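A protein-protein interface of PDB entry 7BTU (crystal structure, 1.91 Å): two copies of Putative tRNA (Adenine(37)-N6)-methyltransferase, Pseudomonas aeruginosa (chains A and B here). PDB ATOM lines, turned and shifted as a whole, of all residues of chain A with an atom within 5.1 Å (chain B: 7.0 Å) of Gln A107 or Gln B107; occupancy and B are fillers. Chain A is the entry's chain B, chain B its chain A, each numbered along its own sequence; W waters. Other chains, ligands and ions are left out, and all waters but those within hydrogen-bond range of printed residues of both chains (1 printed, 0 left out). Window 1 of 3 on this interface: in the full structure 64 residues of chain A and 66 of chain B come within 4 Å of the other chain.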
ATOM      1  N   TRP A  63     -15.167  -7.839  -2.662  1.00  0.00           N
ATOM      2  CA  TRP A  63     -14.083  -8.287  -1.807  1.00  0.00           C
ATOM      3  C   TRP A  63     -12.775  -7.892  -2.443  1.00  0.00           C
ATOM      4  O   TRP A  63     -12.572  -8.146  -3.639  1.00  0.00           O
ATOM      5  CB  TRP A  63     -14.144  -9.809  -1.659  1.00  0.00           C
ATOM      6  CG  TRP A  63     -15.213 -10.335  -0.729  1.00  0.00           C
ATOM      7  CD1 TRP A  63     -16.338 -11.044  -1.072  1.00  0.00           C
ATOM      8  CD2 TRP A  63     -15.202 -10.270   0.710  1.00  0.00           C
ATOM      9  NE1 TRP A  63     -17.013 -11.404   0.046  1.00  0.00           N
ATOM     10  CE2 TRP A  63     -16.347 -10.939   1.156  1.00  0.00           C
ATOM     11  CE3 TRP A  63     -14.301  -9.709   1.666  1.00  0.00           C
ATOM     12  CZ2 TRP A  63     -16.676 -11.062   2.532  1.00  0.00           C
ATOM     13  CZ3 TRP A  63     -14.598  -9.851   3.022  1.00  0.00           C
ATOM     14  CH2 TRP A  63     -15.801 -10.527   3.442  1.00  0.00           C
ATOM     15  N   LEU A  64     -11.861  -7.326  -1.641  1.00  0.00           N
ATOM     16  CA  LEU A  64     -10.495  -7.108  -2.065  1.00  0.00           C
ATOM     17  C   LEU A  64      -9.599  -7.965  -1.177  1.00  0.00           C
ATOM     18  O   LEU A  64      -9.677  -7.880   0.057  1.00  0.00           O
ATOM     19  CB  LEU A  64     -10.080  -5.620  -1.962  1.00  0.00           C
ATOM     20  CG  LEU A  64     -10.900  -4.588  -2.778  1.00  0.00           C
ATOM     21  CD1 LEU A  64     -10.411  -3.134  -2.555  1.00  0.00           C
ATOM     22  CD2 LEU A  64     -10.969  -4.974  -4.300  1.00  0.00           C
ATOM     23  N   LEU A  65      -8.742  -8.755  -1.789  1.00  0.00           N
ATOM     24  CA  LEU A  65      -7.629  -9.380  -1.086  1.00  0.00           C
ATOM     25  C   LEU A  65      -6.427  -8.484  -1.320  1.00  0.00           C
ATOM     26  O   LEU A  65      -6.190  -8.021  -2.457  1.00  0.00           O
ATOM     27  CB  LEU A  65      -7.293 -10.798  -1.624  1.00  0.00           C
ATOM     28  CG  LEU A  65      -8.447 -11.777  -1.503  1.00  0.00           C
ATOM     29  CD1 LEU A  65      -8.131 -13.143  -2.117  1.00  0.00           C
ATOM     30  CD2 LEU A  65      -8.920 -11.934  -0.045  1.00  0.00           C
ATOM     31  N   PHE A  66      -5.643  -8.271  -0.257  1.00  0.00           N
ATOM     32  CA  PHE A  66      -4.580  -7.292  -0.317  1.00  0.00           C
ATOM     33  C   PHE A  66      -3.435  -7.734   0.575  1.00  0.00           C
ATOM     34  O   PHE A  66      -3.540  -8.685   1.360  1.00  0.00           O
ATOM     35  CB  PHE A  66      -5.106  -5.907   0.093  1.00  0.00           C
ATOM     36  CG  PHE A  66      -5.549  -5.856   1.541  1.00  0.00           C
ATOM     37  CD1 PHE A  66      -6.889  -6.124   1.888  1.00  0.00           C
ATOM     38  CD2 PHE A  66      -4.635  -5.528   2.528  1.00  0.00           C
ATOM     39  CE1 PHE A  66      -7.287  -6.090   3.264  1.00  0.00           C
ATOM     40  CE2 PHE A  66      -4.984  -5.471   3.915  1.00  0.00           C
ATOM     41  CZ  PHE A  66      -6.327  -5.749   4.270  1.00  0.00           C
ATOM     42  N   ARG A  97      -8.144 -10.753  13.345  1.00  0.00           N
ATOM     43  CA  ARG A  97      -7.840 -10.111  12.079  1.00  0.00           C
ATOM     44  C   ARG A  97      -6.595  -9.236  12.202  1.00  0.00           C
ATOM     45  O   ARG A  97      -6.470  -8.223  11.501  1.00  0.00           O
ATOM     46  CB  ARG A  97      -9.042  -9.288  11.615  1.00  0.00           C
ATOM     47  CG  ARG A  97     -10.279 -10.098  11.370  1.00  0.00           C
ATOM     48  CD  ARG A  97     -11.467  -9.163  11.191  1.00  0.00           C
ATOM     49  NE  ARG A  97     -12.645  -9.923  10.798  1.00  0.00           N
ATOM     50  CZ  ARG A  97     -12.845 -10.457   9.597  1.00  0.00           C
ATOM     51  NH1 ARG A  97     -11.950 -10.299   8.609  1.00  0.00           N
ATOM     52  NH2 ARG A  97     -13.936 -11.149   9.392  1.00  0.00           N
ATOM     53  N   ILE A 105      -1.742 -11.585   4.091  1.00  0.00           N
ATOM     54  CA  ILE A 105      -2.859 -11.237   3.208  1.00  0.00           C
ATOM     55  C   ILE A 105      -4.074 -10.845   4.038  1.00  0.00           C
ATOM     56  O   ILE A 105      -4.411 -11.535   4.994  1.00  0.00           O
ATOM     57  CB  ILE A 105      -3.219 -12.415   2.282  1.00  0.00           C
ATOM     58  CG1 ILE A 105      -2.038 -12.751   1.392  1.00  0.00           C
ATOM     59  CG2 ILE A 105      -4.419 -12.026   1.343  1.00  0.00           C
ATOM     60  CD1 ILE A 105      -2.205 -14.056   0.778  1.00  0.00           C
ATOM     61  N   GLY A 106      -4.731  -9.741   3.672  1.00  0.00           N
ATOM     62  CA  GLY A 106      -5.939  -9.313   4.339  1.00  0.00           C
ATOM     63  C   GLY A 106      -7.094  -9.396   3.365  1.00  0.00           C
ATOM     64  O   GLY A 106      -6.903  -9.542   2.166  1.00  0.00           O
ATOM     65  N   GLN A 107      -8.302  -9.228   3.900  1.00  0.00           N
ATOM     66  CA  GLN A 107      -9.473  -9.236   3.043  1.00  0.00           C
ATOM     67  C   GLN A 107     -10.329  -8.071   3.491  1.00  0.00           C
ATOM     68  O   GLN A 107     -10.320  -7.720   4.674  1.00  0.00           O
ATOM     69  CB  GLN A 107     -10.258 -10.511   3.151  1.00  0.00           C
ATOM     70  CG  GLN A 107     -10.753 -10.704   4.591  1.00  0.00           C
ATOM     71  CD  GLN A 107     -11.499 -11.984   4.782  1.00  0.00           C
ATOM     72  OE1 GLN A 107     -11.104 -13.050   4.269  1.00  0.00           O
ATOM     73  NE2 GLN A 107     -12.622 -11.892   5.486  1.00  0.00           N
ATOM     74  N   SER A 108     -10.994  -7.417   2.543  1.00  0.00           N
ATOM     75  CA  SER A 108     -11.949  -6.433   3.006  1.00  0.00           C
ATOM     76  C   SER A 108     -13.107  -6.326   2.014  1.00  0.00           C
ATOM     77  O   SER A 108     -12.940  -6.556   0.805  1.00  0.00           O
ATOM     78  CB  SER A 108     -11.257  -5.101   3.263  1.00  0.00           C
ATOM     79  OG  SER A 108     -11.173  -4.313   2.125  1.00  0.00           O
ATOM     80  N   VAL A 109     -14.295  -6.007   2.546  1.00  0.00           N
ATOM     81  CA  VAL A 109     -15.475  -5.781   1.711  1.00  0.00           C
ATOM     82  C   VAL A 109     -15.675  -4.285   1.656  1.00  0.00           C
ATOM     83  O   VAL A 109     -15.579  -3.599   2.688  1.00  0.00           O
ATOM     84  CB  VAL A 109     -16.728  -6.525   2.219  1.00  0.00           C
ATOM     85  CG1 VAL A 109     -16.952  -6.340   3.706  1.00  0.00           C
ATOM     86  CG2 VAL A 109     -17.983  -6.052   1.446  1.00  0.00           C
ATOM     87  N   TRP B  63     -13.167 -17.682   7.892  1.00  0.00           N
ATOM     88  CA  TRP B  63     -12.704 -17.514   6.515  1.00  0.00           C
ATOM     89  C   TRP B  63     -11.444 -18.319   6.320  1.00  0.00           C
ATOM     90  O   TRP B  63     -10.508 -18.226   7.130  1.00  0.00           O
ATOM     91  CB  TRP B  63     -12.347 -16.055   6.262  1.00  0.00           C
ATOM     92  CG  TRP B  63     -13.552 -15.174   6.284  1.00  0.00           C
ATOM     93  CD1 TRP B  63     -13.941 -14.308   7.288  1.00  0.00           C
ATOM     94  CD2 TRP B  63     -14.561 -15.086   5.255  1.00  0.00           C
ATOM     95  NE1 TRP B  63     -15.124 -13.656   6.930  1.00  0.00           N
ATOM     96  CE2 TRP B  63     -15.511 -14.107   5.683  1.00  0.00           C
ATOM     97  CE3 TRP B  63     -14.735 -15.711   4.004  1.00  0.00           C
ATOM     98  CZ2 TRP B  63     -16.629 -13.769   4.915  1.00  0.00           C
ATOM     99  CZ3 TRP B  63     -15.859 -15.370   3.230  1.00  0.00           C
ATOM    100  CH2 TRP B  63     -16.780 -14.426   3.687  1.00  0.00           C
ATOM    101  N   LEU B  64     -11.368 -19.033   5.194  1.00  0.00           N
ATOM    102  CA  LEU B  64     -10.135 -19.677   4.780  1.00  0.00           C
ATOM    103  C   LEU B  64      -9.669 -18.987   3.515  1.00  0.00           C
ATOM    104  O   LEU B  64     -10.472 -18.792   2.581  1.00  0.00           O
ATOM    105  CB  LEU B  64     -10.334 -21.173   4.490  1.00  0.00           C
ATOM    106  CG  LEU B  64     -10.824 -21.988   5.696  1.00  0.00           C
ATOM    107  CD1 LEU B  64     -11.008 -23.462   5.260  1.00  0.00           C
ATOM    108  CD2 LEU B  64      -9.780 -21.855   6.925  1.00  0.00           C
ATOM    109  N   LEU B  65      -8.405 -18.566   3.496  1.00  0.00           N
ATOM    110  CA  LEU B  65      -7.765 -18.193   2.244  1.00  0.00           C
ATOM    111  C   LEU B  65      -6.979 -19.404   1.758  1.00  0.00           C
ATOM    112  O   LEU B  65      -6.308 -20.067   2.554  1.00  0.00           O
ATOM    113  CB  LEU B  65      -6.802 -17.017   2.386  1.00  0.00           C
ATOM    114  CG  LEU B  65      -7.500 -15.742   2.926  1.00  0.00           C
ATOM    115  CD1 LEU B  65      -6.462 -14.627   2.963  1.00  0.00           C
ATOM    116  CD2 LEU B  65      -8.725 -15.259   2.097  1.00  0.00           C
ATOM    117  N   PHE B  66      -7.067 -19.696   0.462  1.00  0.00           N
ATOM    118  CA  PHE B  66      -6.492 -20.949  -0.009  1.00  0.00           C
ATOM    119  C   PHE B  66      -5.963 -20.775  -1.430  1.00  0.00           C
ATOM    120  O   PHE B  66      -6.298 -19.820  -2.149  1.00  0.00           O
ATOM    121  CB  PHE B  66      -7.535 -22.083   0.113  1.00  0.00           C
ATOM    122  CG  PHE B  66      -8.787 -21.824  -0.704  1.00  0.00           C
ATOM    123  CD1 PHE B  66      -8.835 -22.223  -2.047  1.00  0.00           C
ATOM    124  CD2 PHE B  66      -9.879 -21.216  -0.147  1.00  0.00           C
ATOM    125  CE1 PHE B  66      -9.956 -21.981  -2.838  1.00  0.00           C
ATOM    126  CE2 PHE B  66     -11.053 -20.955  -0.922  1.00  0.00           C
ATOM    127  CZ  PHE B  66     -11.085 -21.331  -2.270  1.00  0.00           C
ATOM    128  N   PHE B  68      -6.104 -22.078  -5.228  1.00  0.00           N
ATOM    129  CA  PHE B  68      -6.811 -22.972  -6.145  1.00  0.00           C
ATOM    130  C   PHE B  68      -5.777 -23.930  -6.722  1.00  0.00           C
ATOM    131  O   PHE B  68      -5.143 -23.581  -7.704  1.00  0.00           O
ATOM    132  CB  PHE B  68      -7.478 -22.193  -7.270  1.00  0.00           C
ATOM    133  CG  PHE B  68      -8.639 -21.349  -6.830  1.00  0.00           C
ATOM    134  CD1 PHE B  68      -9.873 -21.924  -6.569  1.00  0.00           C
ATOM    135  CD2 PHE B  68      -8.504 -19.980  -6.698  1.00  0.00           C
ATOM    136  CE1 PHE B  68     -10.947 -21.149  -6.163  1.00  0.00           C
ATOM    137  CE2 PHE B  68      -9.588 -19.192  -6.280  1.00  0.00           C
ATOM    138  CZ  PHE B  68     -10.812 -19.784  -6.020  1.00  0.00           C
ATOM    139  N   ARG B  97     -16.742 -15.189  -9.265  1.00  0.00           N
ATOM    140  CA  ARG B  97     -16.129 -15.968  -8.198  1.00  0.00           C
ATOM    141  C   ARG B  97     -15.547 -17.250  -8.790  1.00  0.00           C
ATOM    142  O   ARG B  97     -15.590 -18.314  -8.174  1.00  0.00           O
ATOM    143  CB  ARG B  97     -17.159 -16.260  -7.099  1.00  0.00           C
ATOM    144  CG  ARG B  97     -17.626 -14.982  -6.340  1.00  0.00           C
ATOM    145  CD  ARG B  97     -18.975 -15.128  -5.603  1.00  0.00           C
ATOM    146  NE  ARG B  97     -18.904 -15.826  -4.309  1.00  0.00           N
ATOM    147  CZ  ARG B  97     -18.701 -15.275  -3.096  1.00  0.00           C
ATOM    148  NH1 ARG B  97     -18.484 -13.936  -2.916  1.00  0.00           N
ATOM    149  NH2 ARG B  97     -18.675 -16.104  -2.035  1.00  0.00           N
ATOM    150  N   ARG B 101      -8.255 -17.302 -11.103  1.00  0.00           N
ATOM    151  CA  ARG B 101      -8.091 -15.904 -10.699  1.00  0.00           C
ATOM    152  C   ARG B 101      -6.630 -15.526 -10.878  1.00  0.00           C
ATOM    153  O   ARG B 101      -5.734 -16.371 -10.708  1.00  0.00           O
ATOM    154  CB  ARG B 101      -8.490 -15.669  -9.239  1.00  0.00           C
ATOM    155  CG  ARG B 101      -9.728 -16.413  -8.865  1.00  0.00           C
ATOM    156  CD  ARG B 101     -10.496 -15.769  -7.807  1.00  0.00           C
ATOM    157  NE  ARG B 101     -10.877 -14.392  -8.131  1.00  0.00           N
ATOM    158  CZ  ARG B 101     -11.907 -14.043  -8.894  1.00  0.00           C
ATOM    159  NH1 ARG B 101     -12.690 -14.976  -9.483  1.00  0.00           N
ATOM    160  NH2 ARG B 101     -12.134 -12.753  -9.101  1.00  0.00           N
ATOM    161  N   ILE B 105      -5.603 -17.211  -5.622  1.00  0.00           N
ATOM    162  CA  ILE B 105      -6.016 -17.282  -4.213  1.00  0.00           C
ATOM    163  C   ILE B 105      -7.528 -17.212  -4.123  1.00  0.00           C
ATOM    164  O   ILE B 105      -8.146 -16.280  -4.656  1.00  0.00           O
ATOM    165  CB  ILE B 105      -5.368 -16.162  -3.387  1.00  0.00           C
ATOM    166  CG1 ILE B 105      -3.879 -16.442  -3.373  1.00  0.00           C
ATOM    167  CG2 ILE B 105      -5.900 -16.194  -1.911  1.00  0.00           C
ATOM    168  CD1 ILE B 105      -3.022 -15.318  -2.775  1.00  0.00           C
ATOM    169  N   GLY B 106      -8.125 -18.162  -3.401  1.00  0.00           N
ATOM    170  CA  GLY B 106      -9.543 -18.126  -3.122  1.00  0.00           C
ATOM    171  C   GLY B 106      -9.824 -17.833  -1.653  1.00  0.00           C
ATOM    172  O   GLY B 106      -8.957 -17.892  -0.778  1.00  0.00           O
ATOM    173  N   GLN B 107     -11.101 -17.555  -1.401  1.00  0.00           N
ATOM    174  CA  GLN B 107     -11.586 -17.217  -0.086  1.00  0.00           C
ATOM    175  C   GLN B 107     -12.927 -17.922   0.107  1.00  0.00           C
ATOM    176  O   GLN B 107     -13.812 -17.821  -0.751  1.00  0.00           O
ATOM    177  CB  GLN B 107     -11.711 -15.664  -0.018  1.00  0.00           C
ATOM    178  CG  GLN B 107     -12.434 -15.155   1.184  1.00  0.00           C
ATOM    179  CD  GLN B 107     -12.681 -13.648   1.135  1.00  0.00           C
ATOM    180  OE1 GLN B 107     -12.154 -12.932   0.261  1.00  0.00           O
ATOM    181  NE2 GLN B 107     -13.483 -13.156   2.084  1.00  0.00           N
ATOM    182  N   SER B 108     -13.131 -18.569   1.248  1.00  0.00           N
ATOM    183  CA  SER B 108     -14.458 -19.127   1.504  1.00  0.00           C
ATOM    184  C   SER B 108     -14.724 -19.072   2.994  1.00  0.00           C
ATOM    185  O   SER B 108     -13.788 -18.982   3.777  1.00  0.00           O
ATOM    186  CB  SER B 108     -14.584 -20.579   1.048  1.00  0.00           C
ATOM    187  OG  SER B 108     -13.774 -21.358   1.924  1.00  0.00           O
ATOM    188  N   VAL B 109     -15.997 -19.018   3.380  1.00  0.00           N
ATOM    189  CA  VAL B 109     -16.353 -19.117   4.794  1.00  0.00           C
ATOM    190  C   VAL B 109     -16.941 -20.503   5.035  1.00  0.00           C
ATOM    191  O   VAL B 109     -17.748 -20.983   4.235  1.00  0.00           O
ATOM    192  CB  VAL B 109     -17.328 -18.016   5.228  1.00  0.00           C
ATOM    193  CG1 VAL B 109     -18.571 -18.020   4.311  1.00  0.00           C
ATOM    194  CG2 VAL B 109     -17.739 -18.201   6.705  1.00  0.00           C
ATOM    195  N   ASP B 126     -16.629 -26.195   0.596  1.00  0.00           N
ATOM    196  CA  ASP B 126     -16.655 -26.471  -0.838  1.00  0.00           C
ATOM    197  C   ASP B 126     -15.254 -26.663  -1.394  1.00  0.00           C
ATOM    198  O   ASP B 126     -15.039 -26.475  -2.581  1.00  0.00           O
ATOM    199  CB  ASP B 126     -17.406 -25.388  -1.620  1.00  0.00           C
ATOM    200  CG  ASP B 126     -16.739 -24.005  -1.583  1.00  0.00           C
ATOM    201  OD1 ASP B 126     -15.692 -23.847  -0.953  1.00  0.00           O
ATOM    202  OD2 ASP B 126     -17.312 -23.066  -2.229  1.00  0.00           O
ATOM    203  N   LEU B 127     -14.303 -27.070  -0.571  1.00  0.00           N
ATOM    204  CA  LEU B 127     -12.912 -27.158  -0.999  1.00  0.00           C
ATOM    205  C   LEU B 127     -12.561 -28.593  -1.371  1.00  0.00           C
ATOM    206  O   LEU B 127     -13.002 -29.532  -0.714  1.00  0.00           O
ATOM    207  CB  LEU B 127     -11.942 -26.723   0.120  1.00  0.00           C
ATOM    208  CG  LEU B 127     -12.181 -25.278   0.675  1.00  0.00           C
ATOM    209  CD1 LEU B 127     -11.055 -24.876   1.669  1.00  0.00           C
ATOM    210  CD2 LEU B 127     -12.210 -24.290  -0.489  1.00  0.00           C
ATOM    211  N   LYS B 137      -9.159 -16.808   9.295  1.00  0.00           N
ATOM    212  CA  LYS B 137      -9.628 -15.593   9.965  1.00  0.00           C
ATOM    213  C   LYS B 137     -10.988 -15.878  10.579  1.00  0.00           C
ATOM    214  O   LYS B 137     -11.812 -16.520   9.929  1.00  0.00           O
ATOM    215  CB  LYS B 137      -9.761 -14.418   8.977  1.00  0.00           C
ATOM    216  CG  LYS B 137      -8.436 -13.989   8.308  1.00  0.00           C
ATOM    217  CD  LYS B 137      -8.698 -12.921   7.182  1.00  0.00           C
ATOM    218  CE  LYS B 137      -7.407 -12.189   6.790  1.00  0.00           C
ATOM    219  NZ  LYS B 137      -6.487 -13.063   6.158  1.00  0.00           N
ATOM    220  N   PRO B 138     -11.278 -15.370  11.787  1.00  0.00           N
ATOM    221  CA  PRO B 138     -12.639 -15.506  12.328  1.00  0.00           C
ATOM    222  C   PRO B 138     -13.634 -14.737  11.469  1.00  0.00           C
ATOM    223  O   PRO B 138     -13.335 -13.658  10.949  1.00  0.00           O
ATOM    224  CB  PRO B 138     -12.539 -14.888  13.749  1.00  0.00           C
ATOM    225  CG  PRO B 138     -11.381 -13.863  13.585  1.00  0.00           C
ATOM    226  CD  PRO B 138     -10.402 -14.549  12.650  1.00  0.00           C
ATOM    227  N   TYR B 139     -14.823 -15.299  11.322  1.00  0.00           N
ATOM    228  CA  TYR B 139     -15.920 -14.564  10.711  1.00  0.00           C
ATOM    229  C   TYR B 139     -16.457 -13.580  11.758  1.00  0.00           C
ATOM    230  O   TYR B 139     -16.765 -13.966  12.900  1.00  0.00           O
ATOM    231  CB  TYR B 139     -17.025 -15.532  10.273  1.00  0.00           C
ATOM    232  CG  TYR B 139     -18.107 -14.875   9.456  1.00  0.00           C
ATOM    233  CD1 TYR B 139     -19.193 -14.290  10.075  1.00  0.00           C
ATOM    234  CD2 TYR B 139     -18.037 -14.850   8.066  1.00  0.00           C
ATOM    235  CE1 TYR B 139     -20.198 -13.653   9.316  1.00  0.00           C
ATOM    236  CE2 TYR B 139     -19.046 -14.246   7.294  1.00  0.00           C
ATOM    237  CZ  TYR B 139     -20.099 -13.631   7.925  1.00  0.00           C
ATOM    238  OH  TYR B 139     -21.054 -12.973   7.180  1.00  0.00           O
ATOM    239  N   ASP B 144     -18.563  -8.413   8.369  1.00  0.00           N
ATOM    240  CA  ASP B 144     -18.536  -9.265   7.178  1.00  0.00           C
ATOM    241  C   ASP B 144     -19.901  -9.489   6.541  1.00  0.00           C
ATOM    242  O   ASP B 144     -19.957  -9.897   5.380  1.00  0.00           O
ATOM    243  CB  ASP B 144     -17.986 -10.669   7.517  1.00  0.00           C
ATOM    244  CG  ASP B 144     -16.545 -10.655   7.969  1.00  0.00           C
ATOM    245  OD1 ASP B 144     -15.833  -9.662   7.725  1.00  0.00           O
ATOM    246  OD2 ASP B 144     -16.128 -11.649   8.601  1.00  0.00           O
HETATM  247  O   HOH W   1     -13.474  -9.360   6.469  1.00  0.00           O
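The indole nitrogen (NE1) of Trp B63 sits at hydrogen-bond distance from the side-chain carboxylate (OD2) of Asp B144 (2.8 Å).
The backbone carbonyl oxygen (O) of Lys B137 sits at hydrogen-bond distance from the backbone NH (N) of Trp B63 (2.7 Å).
Trp B63 touches its own counterpart, Trp A63.
Trp A63 touches Gln B107, and with the chains exchanged Gln A107 touches Trp B63.
Leu A65 touches Gln B107, and with the chains exchanged Gln A107 touches Leu B65.
Arg A97 touches Trp B63, but with the chains exchanged Trp A63 does not touch Arg B97 (4.05 Å).
Of the 15 pairs that touch across the chains among the printed residues, 10 have their exchanged pair printed and touching as well.
The side-chain amide nitrogen (NE2) of Gln B107 is in hydrogen-bond range of the side-chain amide oxygen (OE1) of Gln A107.
NH2 of Arg A97 is in hydrogen-bond range of O of Pro B138.
The side-chain amide nitrogen of Gln A107 lies close to the indole nitrogen of Trp B63 (3.4 Å).
NZ of Lys B137 sits at hydrogen-bond distance from O of Ile A105 (2.8 Å).
The side-chain carboxylate (OD1) of Asp B144 is in salt-bridge range of the guanidinium group (NH2) of Arg A97, 2.9 Å away.
Water W1 lies within hydrogen-bond range of the side-chain carboxylate of Asp B144 (2.7 Å), the guanidinium group of Arg A97 (2.8 Å) and the side-chain amide nitrogen of Gln A107 (2.8 Å).
Trp B63 touches Trp A63.
Trp A63 touches Gln B107 (CE3 to NE2, 3.6 Å).
Leu B65 touches Leu A65.
Leu A65 touches Ile B105 (CD1 to CG2, 3.8 Å).
Leu A65 touches Gln B107 (CD2 to OE1, 3.4 Å).
Trp B63 touches Arg A97.
Ile A105 touches Leu B65 (CG2 to CD1, 3.7 Å).
Ile B105 touches Ile A105.
CD2 of Leu B65 touches OE1 of Gln A107, 3.9 Å away.
CD of Lys B137 touches OE1 of Gln A107 (3.8 Å).
Hydrophobic or aromatic side chains of chain A that line the printed part of chain B: Trp A63, Leu A65 and Ile A105.
Hydrophobic or aromatic side chains of chain B within 4 Å of the printed part of chain A: Trp B63, Leu B65 and Ile B105.
Among the printed residues, 15 pairs touch across the chains.
Among the printed residues, Asp or Glu carboxylates within 4 Å of a Lys or Arg side-chain nitrogen of the other chain: Arg A97 with Asp B144 (2.4 Å).
Of the printed residues of chain B, Ile A105 touches Leu B65, Ile B105 and Lys B137.
Of chain B, only Trp B63 (3.3 Å), Leu B65 (3.9 Å), Gln B107 (3.2 Å) and Lys B137 (3.8 Å) come within 4 Å of Gln A107.
Of the printed residues of chain A, Gln B107 touches Trp A63, Leu A65 and Gln A107.
Of the printed residues of chain A, Lys B137 touches Ile A105 and Gln A107.
Of the printed residues of chain A, Asp B144 touches Arg A97.
The nearest residue of chain B that does not touch Gln A107 is Asp B144 (4.5 Å).
The nearest printed residue of chain B that does not touch Trp A63 is Arg B97 (4.05 Å).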
